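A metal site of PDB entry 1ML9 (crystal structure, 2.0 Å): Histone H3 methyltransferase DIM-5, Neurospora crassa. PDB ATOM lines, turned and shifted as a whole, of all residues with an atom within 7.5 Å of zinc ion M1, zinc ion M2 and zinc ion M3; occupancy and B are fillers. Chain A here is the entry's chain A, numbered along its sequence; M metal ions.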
ATOM      1  N   VAL A  48     -29.562 -11.055  -0.794  1.00  0.00           N
ATOM      2  CA  VAL A  48     -29.018 -11.592  -2.024  1.00  0.00           C
ATOM      3  C   VAL A  48     -27.715 -10.881  -2.425  1.00  0.00           C
ATOM      4  O   VAL A  48     -27.599  -9.652  -2.327  1.00  0.00           O
ATOM      5  CB  VAL A  48     -30.093 -11.518  -3.193  1.00  0.00           C
ATOM      6  CG1 VAL A  48     -31.115 -10.436  -2.911  1.00  0.00           C
ATOM      7  CG2 VAL A  48     -29.430 -11.276  -4.539  1.00  0.00           C
ATOM      8  N   GLY A  49     -26.724 -11.673  -2.844  1.00  0.00           N
ATOM      9  CA  GLY A  49     -25.453 -11.131  -3.282  1.00  0.00           C
ATOM     10  C   GLY A  49     -25.277 -11.423  -4.766  1.00  0.00           C
ATOM     11  O   GLY A  49     -25.868 -12.379  -5.265  1.00  0.00           O
ATOM     12  N   CYS A  50     -24.496 -10.614  -5.479  1.00  0.00           N
ATOM     13  CA  CYS A  50     -24.289 -10.841  -6.909  1.00  0.00           C
ATOM     14  C   CYS A  50     -23.522 -12.141  -7.112  1.00  0.00           C
ATOM     15  O   CYS A  50     -22.848 -12.614  -6.202  1.00  0.00           O
ATOM     16  CB  CYS A  50     -23.533  -9.674  -7.539  1.00  0.00           C
ATOM     17  SG  CYS A  50     -21.804  -9.469  -6.990  1.00  0.00           S
ATOM     18  N   SER A  51     -23.634 -12.708  -8.314  1.00  0.00           N
ATOM     19  CA  SER A  51     -22.953 -13.962  -8.618  1.00  0.00           C
ATOM     20  C   SER A  51     -21.829 -13.777  -9.629  1.00  0.00           C
ATOM     21  O   SER A  51     -21.492 -14.688 -10.380  1.00  0.00           O
ATOM     22  CB  SER A  51     -23.961 -14.983  -9.174  1.00  0.00           C
ATOM     23  OG  SER A  51     -24.610 -14.474 -10.322  1.00  0.00           O
ATOM     24  N   CYS A  52     -21.234 -12.589  -9.626  1.00  0.00           N
ATOM     25  CA  CYS A  52     -20.145 -12.274 -10.545  1.00  0.00           C
ATOM     26  C   CYS A  52     -19.009 -13.284 -10.500  1.00  0.00           C
ATOM     27  O   CYS A  52     -18.578 -13.715  -9.424  1.00  0.00           O
ATOM     28  CB  CYS A  52     -19.625 -10.878 -10.262  1.00  0.00           C
ATOM     29  SG  CYS A  52     -20.765  -9.581 -10.837  1.00  0.00           S
ATOM     30  N   ALA A  53     -18.533 -13.672 -11.693  1.00  0.00           N
ATOM     31  CA  ALA A  53     -17.461 -14.632 -11.802  1.00  0.00           C
ATOM     32  C   ALA A  53     -16.190 -14.175 -11.112  1.00  0.00           C
ATOM     33  O   ALA A  53     -15.603 -14.920 -10.324  1.00  0.00           O
ATOM     34  N   SER A  54     -15.756 -12.951 -11.421  1.00  0.00           N
ATOM     35  CA  SER A  54     -14.553 -12.396 -10.814  1.00  0.00           C
ATOM     36  C   SER A  54     -14.805 -10.962 -10.350  1.00  0.00           C
ATOM     37  O   SER A  54     -15.671 -10.273 -10.893  1.00  0.00           O
ATOM     38  CB  SER A  54     -13.400 -12.425 -11.812  1.00  0.00           C
ATOM     39  N   ASP A  55     -14.041 -10.538  -9.347  1.00  0.00           N
ATOM     40  CA  ASP A  55     -14.152  -9.200  -8.792  1.00  0.00           C
ATOM     41  C   ASP A  55     -14.194  -8.126  -9.867  1.00  0.00           C
ATOM     42  O   ASP A  55     -14.607  -6.997  -9.615  1.00  0.00           O
ATOM     43  CB  ASP A  55     -12.969  -8.923  -7.853  1.00  0.00           C
ATOM     44  CG  ASP A  55     -13.007  -9.792  -6.632  1.00  0.00           C
ATOM     45  OD1 ASP A  55     -13.761 -10.784  -6.648  1.00  0.00           O
ATOM     46  OD2 ASP A  55     -12.309  -9.476  -5.639  1.00  0.00           O
ATOM     47  N   GLU A  56     -13.774  -8.471 -11.079  1.00  0.00           N
ATOM     48  CA  GLU A  56     -13.753  -7.524 -12.176  1.00  0.00           C
ATOM     49  C   GLU A  56     -15.135  -7.277 -12.797  1.00  0.00           C
ATOM     50  O   GLU A  56     -15.437  -6.148 -13.202  1.00  0.00           O
ATOM     51  CB  GLU A  56     -12.773  -7.985 -13.239  1.00  0.00           C
ATOM     52  N   GLU A  57     -15.969  -8.311 -12.881  1.00  0.00           N
ATOM     53  CA  GLU A  57     -17.293  -8.147 -13.473  1.00  0.00           C
ATOM     54  C   GLU A  57     -18.220  -7.208 -12.713  1.00  0.00           C
ATOM     55  O   GLU A  57     -19.093  -6.553 -13.299  1.00  0.00           O
ATOM     56  N   CYS A  58     -18.023  -7.135 -11.396  1.00  0.00           N
ATOM     57  CA  CYS A  58     -18.835  -6.306 -10.530  1.00  0.00           C
ATOM     58  C   CYS A  58     -18.907  -4.821 -10.904  1.00  0.00           C
ATOM     59  O   CYS A  58     -19.805  -4.117 -10.436  1.00  0.00           O
ATOM     60  CB  CYS A  58     -18.341  -6.423  -9.085  1.00  0.00           C
ATOM     61  SG  CYS A  58     -18.676  -8.037  -8.306  1.00  0.00           S
ATOM     62  N   MET A  59     -17.987  -4.342 -11.734  1.00  0.00           N
ATOM     63  CA  MET A  59     -18.031  -2.925 -12.113  1.00  0.00           C
ATOM     64  C   MET A  59     -18.834  -2.661 -13.365  1.00  0.00           C
ATOM     65  O   MET A  59     -18.855  -1.537 -13.875  1.00  0.00           O
ATOM     66  CB  MET A  59     -16.622  -2.348 -12.277  1.00  0.00           C
ATOM     67  CG  MET A  59     -15.559  -3.312 -12.737  1.00  0.00           C
ATOM     68  SD  MET A  59     -13.922  -2.540 -12.735  1.00  0.00           S
ATOM     69  CE  MET A  59     -12.927  -3.828 -11.949  1.00  0.00           C
ATOM     70  N   TYR A  60     -19.521  -3.688 -13.862  1.00  0.00           N
ATOM     71  CA  TYR A  60     -20.335  -3.555 -15.069  1.00  0.00           C
ATOM     72  C   TYR A  60     -21.837  -3.628 -14.794  1.00  0.00           C
ATOM     73  O   TYR A  60     -22.285  -4.140 -13.760  1.00  0.00           O
ATOM     74  CB  TYR A  60     -19.935  -4.619 -16.082  1.00  0.00           C
ATOM     75  CG  TYR A  60     -18.529  -4.454 -16.605  1.00  0.00           C
ATOM     76  CD1 TYR A  60     -17.507  -5.308 -16.181  1.00  0.00           C
ATOM     77  CD2 TYR A  60     -18.221  -3.450 -17.523  1.00  0.00           C
ATOM     78  CE1 TYR A  60     -16.208  -5.154 -16.664  1.00  0.00           C
ATOM     79  CE2 TYR A  60     -16.925  -3.288 -18.008  1.00  0.00           C
ATOM     80  CZ  TYR A  60     -15.919  -4.154 -17.570  1.00  0.00           C
ATOM     81  OH  TYR A  60     -14.636  -4.017 -18.058  1.00  0.00           O
ATOM     82  N   THR A  62     -23.900  -5.527 -15.537  1.00  0.00           N
ATOM     83  CA  THR A  62     -24.395  -6.884 -15.346  1.00  0.00           C
ATOM     84  C   THR A  62     -24.325  -7.366 -13.909  1.00  0.00           C
ATOM     85  O   THR A  62     -24.898  -8.407 -13.559  1.00  0.00           O
ATOM     86  CB  THR A  62     -23.620  -7.886 -16.217  1.00  0.00           C
ATOM     87  OG1 THR A  62     -22.372  -8.211 -15.579  1.00  0.00           O
ATOM     88  CG2 THR A  62     -23.345  -7.306 -17.591  1.00  0.00           C
ATOM     89  N   CYS A  63     -23.618  -6.642 -13.055  1.00  0.00           N
ATOM     90  CA  CYS A  63     -23.523  -7.042 -11.662  1.00  0.00           C
ATOM     91  C   CYS A  63     -24.916  -6.868 -11.042  1.00  0.00           C
ATOM     92  O   CYS A  63     -25.564  -5.830 -11.221  1.00  0.00           O
ATOM     93  CB  CYS A  63     -22.482  -6.185 -10.941  1.00  0.00           C
ATOM     94  SG  CYS A  63     -22.339  -6.516  -9.154  1.00  0.00           S
ATOM     95  N   GLN A  64     -25.378  -7.893 -10.329  1.00  0.00           N
ATOM     96  CA  GLN A  64     -26.690  -7.848  -9.680  1.00  0.00           C
ATOM     97  C   GLN A  64     -26.827  -6.669  -8.740  1.00  0.00           C
ATOM     98  O   GLN A  64     -27.878  -6.032  -8.661  1.00  0.00           O
ATOM     99  CB  GLN A  64     -26.924  -9.139  -8.887  1.00  0.00           C
ATOM    100  CG  GLN A  64     -27.687 -10.191  -9.652  1.00  0.00           C
ATOM    101  CD  GLN A  64     -26.779 -11.276 -10.198  1.00  0.00           C
ATOM    102  OE1 GLN A  64     -25.605 -11.369  -9.834  1.00  0.00           O
ATOM    103  NE2 GLN A  64     -27.324 -12.112 -11.092  1.00  0.00           N
ATOM    104  N   CYS A  65     -25.747  -6.383  -8.027  1.00  0.00           N
ATOM    105  CA  CYS A  65     -25.701  -5.293  -7.062  1.00  0.00           C
ATOM    106  C   CYS A  65     -26.023  -3.934  -7.640  1.00  0.00           C
ATOM    107  O   CYS A  65     -26.613  -3.089  -6.974  1.00  0.00           O
ATOM    108  CB  CYS A  65     -24.331  -5.285  -6.393  1.00  0.00           C
ATOM    109  SG  CYS A  65     -24.133  -6.746  -5.338  1.00  0.00           S
ATOM    110  N   LEU A  66     -25.642  -3.734  -8.899  1.00  0.00           N
ATOM    111  CA  LEU A  66     -25.888  -2.456  -9.553  1.00  0.00           C
ATOM    112  C   LEU A  66     -27.214  -2.472 -10.304  1.00  0.00           C
ATOM    113  O   LEU A  66     -27.524  -1.538 -11.051  1.00  0.00           O
ATOM    114  CB  LEU A  66     -24.727  -2.147 -10.495  1.00  0.00           C
ATOM    115  CG  LEU A  66     -23.348  -1.889  -9.871  1.00  0.00           C
ATOM    116  CD1 LEU A  66     -22.794  -3.131  -9.189  1.00  0.00           C
ATOM    117  CD2 LEU A  66     -22.408  -1.451 -10.981  1.00  0.00           C
ATOM    118  N   TYR A 110     -24.433   1.892  -4.590  1.00  0.00           N
ATOM    119  CA  TYR A 110     -24.736   0.466  -4.431  1.00  0.00           C
ATOM    120  C   TYR A 110     -23.446  -0.350  -4.485  1.00  0.00           C
ATOM    121  O   TYR A 110     -22.827  -0.482  -5.555  1.00  0.00           O
ATOM    122  CB  TYR A 110     -25.704   0.021  -5.532  1.00  0.00           C
ATOM    123  CG  TYR A 110     -27.090   0.591  -5.358  1.00  0.00           C
ATOM    124  CD1 TYR A 110     -27.453   1.778  -5.972  1.00  0.00           C
ATOM    125  CD2 TYR A 110     -28.030  -0.050  -4.547  1.00  0.00           C
ATOM    126  CE1 TYR A 110     -28.720   2.331  -5.799  1.00  0.00           C
ATOM    127  CE2 TYR A 110     -29.290   0.489  -4.350  1.00  0.00           C
ATOM    128  CZ  TYR A 110     -29.636   1.677  -4.985  1.00  0.00           C
ATOM    129  OH  TYR A 110     -30.887   2.213  -4.809  1.00  0.00           O
ATOM    130  N   GLU A 111     -23.052  -0.882  -3.340  1.00  0.00           N
ATOM    131  CA  GLU A 111     -21.833  -1.662  -3.203  1.00  0.00           C
ATOM    132  C   GLU A 111     -22.075  -3.149  -3.021  1.00  0.00           C
ATOM    133  O   GLU A 111     -23.213  -3.588  -2.801  1.00  0.00           O
ATOM    134  CB  GLU A 111     -21.040  -1.175  -1.981  1.00  0.00           C
ATOM    135  CG  GLU A 111     -20.287   0.124  -2.158  1.00  0.00           C
ATOM    136  CD  GLU A 111     -19.166   0.270  -1.152  1.00  0.00           C
ATOM    137  OE1 GLU A 111     -18.316   1.163  -1.352  1.00  0.00           O
ATOM    138  OE2 GLU A 111     -19.115  -0.491  -0.169  1.00  0.00           O
ATOM    139  N   CYS A 112     -21.000  -3.923  -3.117  1.00  0.00           N
ATOM    140  CA  CYS A 112     -21.098  -5.346  -2.896  1.00  0.00           C
ATOM    141  C   CYS A 112     -21.110  -5.490  -1.378  1.00  0.00           C
ATOM    142  O   CYS A 112     -20.899  -4.499  -0.664  1.00  0.00           O
ATOM    143  CB  CYS A 112     -19.919  -6.083  -3.534  1.00  0.00           C
ATOM    144  SG  CYS A 112     -20.225  -6.380  -5.315  1.00  0.00           S
ATOM    145  N   HIS A 113     -21.349  -6.691  -0.867  1.00  0.00           N
ATOM    146  CA  HIS A 113     -21.472  -6.844   0.575  1.00  0.00           C
ATOM    147  C   HIS A 113     -21.426  -8.296   0.984  1.00  0.00           C
ATOM    148  O   HIS A 113     -21.179  -9.180   0.148  1.00  0.00           O
ATOM    149  CB  HIS A 113     -22.839  -6.288   0.970  1.00  0.00           C
ATOM    150  CG  HIS A 113     -23.922  -6.669   0.012  1.00  0.00           C
ATOM    151  ND1 HIS A 113     -24.142  -5.986  -1.170  1.00  0.00           N
ATOM    152  CD2 HIS A 113     -24.764  -7.720  -0.005  1.00  0.00           C
ATOM    153  CE1 HIS A 113     -25.079  -6.601  -1.866  1.00  0.00           C
ATOM    154  NE2 HIS A 113     -25.473  -7.655  -1.179  1.00  0.00           N
ATOM    155  N   GLY A 115     -22.195 -11.705   1.196  1.00  0.00           N
ATOM    156  CA  GLY A 115     -23.074 -12.479   0.353  1.00  0.00           C
ATOM    157  C   GLY A 115     -22.634 -12.574  -1.091  1.00  0.00           C
ATOM    158  O   GLY A 115     -22.847 -13.602  -1.734  1.00  0.00           O
ATOM    159  N   CYS A 116     -22.012 -11.516  -1.604  1.00  0.00           N
ATOM    160  CA  CYS A 116     -21.546 -11.525  -2.989  1.00  0.00           C
ATOM    161  C   CYS A 116     -20.478 -12.580  -3.259  1.00  0.00           C
ATOM    162  O   CYS A 116     -19.688 -12.919  -2.380  1.00  0.00           O
ATOM    163  CB  CYS A 116     -21.016 -10.151  -3.372  1.00  0.00           C
ATOM    164  SG  CYS A 116     -22.320  -8.900  -3.411  1.00  0.00           S
ATOM    165  N   ALA A 117     -20.461 -13.063  -4.499  1.00  0.00           N
ATOM    166  CA  ALA A 117     -19.514 -14.089  -4.938  1.00  0.00           C
ATOM    167  C   ALA A 117     -18.112 -13.531  -5.211  1.00  0.00           C
ATOM    168  O   ALA A 117     -17.208 -14.269  -5.608  1.00  0.00           O
ATOM    169  CB  ALA A 117     -20.046 -14.784  -6.190  1.00  0.00           C
ATOM    170  N   CYS A 118     -17.955 -12.224  -5.021  1.00  0.00           N
ATOM    171  CA  CYS A 118     -16.662 -11.588  -5.237  1.00  0.00           C
ATOM    172  C   CYS A 118     -15.900 -11.633  -3.916  1.00  0.00           C
ATOM    173  O   CYS A 118     -16.446 -12.058  -2.890  1.00  0.00           O
ATOM    174  CB  CYS A 118     -16.857 -10.150  -5.697  1.00  0.00           C
ATOM    175  SG  CYS A 118     -17.936  -9.165  -4.611  1.00  0.00           S
ATOM    176  N   SER A 119     -14.645 -11.195  -3.933  1.00  0.00           N
ATOM    177  CA  SER A 119     -13.844 -11.203  -2.727  1.00  0.00           C
ATOM    178  C   SER A 119     -13.776  -9.855  -2.048  1.00  0.00           C
ATOM    179  O   SER A 119     -14.181  -8.843  -2.624  1.00  0.00           O
ATOM    180  N   ASP A 121     -11.665  -8.030  -1.878  1.00  0.00           N
ATOM    181  CA  ASP A 121     -10.935  -7.151  -2.772  1.00  0.00           C
ATOM    182  C   ASP A 121     -11.762  -6.551  -3.894  1.00  0.00           C
ATOM    183  O   ASP A 121     -11.233  -5.826  -4.729  1.00  0.00           O
ATOM    184  CB  ASP A 121      -9.746  -7.906  -3.365  1.00  0.00           C
ATOM    185  N   CYS A 122     -13.060  -6.852  -3.921  1.00  0.00           N
ATOM    186  CA  CYS A 122     -13.920  -6.329  -4.969  1.00  0.00           C
ATOM    187  C   CYS A 122     -13.826  -4.802  -5.072  1.00  0.00           C
ATOM    188  O   CYS A 122     -13.984  -4.099  -4.080  1.00  0.00           O
ATOM    189  CB  CYS A 122     -15.379  -6.731  -4.734  1.00  0.00           C
ATOM    190  SG  CYS A 122     -16.509  -5.975  -5.945  1.00  0.00           S
ATOM    191  N   PRO A 123     -13.586  -4.289  -6.283  1.00  0.00           N
ATOM    192  CA  PRO A 123     -13.474  -2.839  -6.502  1.00  0.00           C
ATOM    193  C   PRO A 123     -14.708  -2.059  -6.058  1.00  0.00           C
ATOM    194  O   PRO A 123     -14.679  -0.834  -5.997  1.00  0.00           O
ATOM    195  CB  PRO A 123     -13.238  -2.712  -8.015  1.00  0.00           C
ATOM    196  CG  PRO A 123     -13.659  -4.026  -8.604  1.00  0.00           C
ATOM    197  CD  PRO A 123     -13.399  -5.055  -7.530  1.00  0.00           C
ATOM    198  N   ASN A 124     -15.781  -2.783  -5.768  1.00  0.00           N
ATOM    199  CA  ASN A 124     -17.022  -2.141  -5.350  1.00  0.00           C
ATOM    200  C   ASN A 124     -17.360  -2.422  -3.906  1.00  0.00           C
ATOM    201  O   ASN A 124     -18.517  -2.618  -3.552  1.00  0.00           O
ATOM    202  CB  ASN A 124     -18.173  -2.590  -6.245  1.00  0.00           C
ATOM    203  CG  ASN A 124     -19.343  -1.641  -6.190  1.00  0.00           C
ATOM    204  OD1 ASN A 124     -19.162  -0.429  -6.111  1.00  0.00           O
ATOM    205  ND2 ASN A 124     -20.554  -2.184  -6.220  1.00  0.00           N
ATOM    206  N   ARG A 125     -16.331  -2.429  -3.062  1.00  0.00           N
ATOM    207  CA  ARG A 125     -16.499  -2.652  -1.630  1.00  0.00           C
ATOM    208  C   ARG A 125     -15.667  -1.624  -0.872  1.00  0.00           C
ATOM    209  O   ARG A 125     -15.296  -1.840   0.275  1.00  0.00           O
ATOM    210  CB  ARG A 125     -16.039  -4.059  -1.242  1.00  0.00           C
ATOM    211  CG  ARG A 125     -16.918  -5.191  -1.754  1.00  0.00           C
ATOM    212  CD  ARG A 125     -16.312  -6.548  -1.428  1.00  0.00           C
ATOM    213  NE  ARG A 125     -17.123  -7.654  -1.919  1.00  0.00           N
ATOM    214  CZ  ARG A 125     -17.750  -8.541  -1.141  1.00  0.00           C
ATOM    215  NH1 ARG A 125     -17.672  -8.450   0.177  1.00  0.00           N
ATOM    216  NH2 ARG A 125     -18.455  -9.522  -1.690  1.00  0.00           N
HETATM  217 ZN    ZN M   1     -22.113  -7.817  -5.359  1.00  0.00          ZN
HETATM  218 ZN    ZN M   2     -18.323  -7.457  -6.084  1.00  0.00          ZN
HETATM  219 ZN    ZN M   3     -20.959  -8.357  -8.861  1.00  0.00          ZN
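N of His 113 lies close to SG of Cys 116 (3.5 Å). The side-chain sulfur (SG) of Cys 63 lies close to the backbone NH (N) of Cys 65 (3.6 Å). The backbone carbonyl oxygen of Cys 118 is in hydrogen-bond range of the guanidinium group of Arg 125 (3.5 Å). The backbone NH of Cys 112 is in hydrogen-bond range of the backbone carbonyl oxygen of Asn 124, at 2.8 Å. The backbone carbonyl oxygen (O) of Cys 50 is in hydrogen-bond range of the backbone NH (N) of Ala 117 (3.0 Å). N of Asn 124 sits close to SG of Cys 122 (3.3 Å). N of Cys 122 lies within hydrogen-bond range of OD2 of Asp 55 (3.2 Å).
Within 4 Å of zinc ion M1: Cys 50, Cys 65, Cys 112 and Cys 116. Along chain A the residues within 4 Å of zinc ion M1 span positions 50 to 116. The nearest printed residue that does not touch zinc ion M1 is Cys 63 (4.02 Å).
Within 4 Å of zinc ion M3: Cys 50, Cys 52, Cys 58 and Cys 63.
Zinc ion M1 is bound by the side-chain sulfur (SG) of Cys 116, the side-chain sulfur (SG) of Cys 65, the side-chain sulfur (SG) of Cys 50 and the side-chain sulfur (SG) of Cys 112. Zinc ion M1 has four donor atoms within binding distance.
Zinc ion M2 is bound by SG of Cys 118, at 2.3 Å. Zinc ion M2 is bound by SG of Cys 112. Zinc ion M2 is bound by SG of Cys 58 (2.3 Å). The side-chain sulfur (SG) of Cys 122 binds zinc ion M2 (2.3 Å). Zinc ion M2 has four donor atoms within binding distance.
Zinc ion M3 is bound by the side-chain sulfur of Cys 63 (2.3 Å), the side-chain sulfur of Cys 52 (2.3 Å), the side-chain sulfur of Cys 50 (2.3 Å) and the side-chain sulfur of Cys 58 (2.4 Å). Zinc ion M3 has four donor atoms within binding distance.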
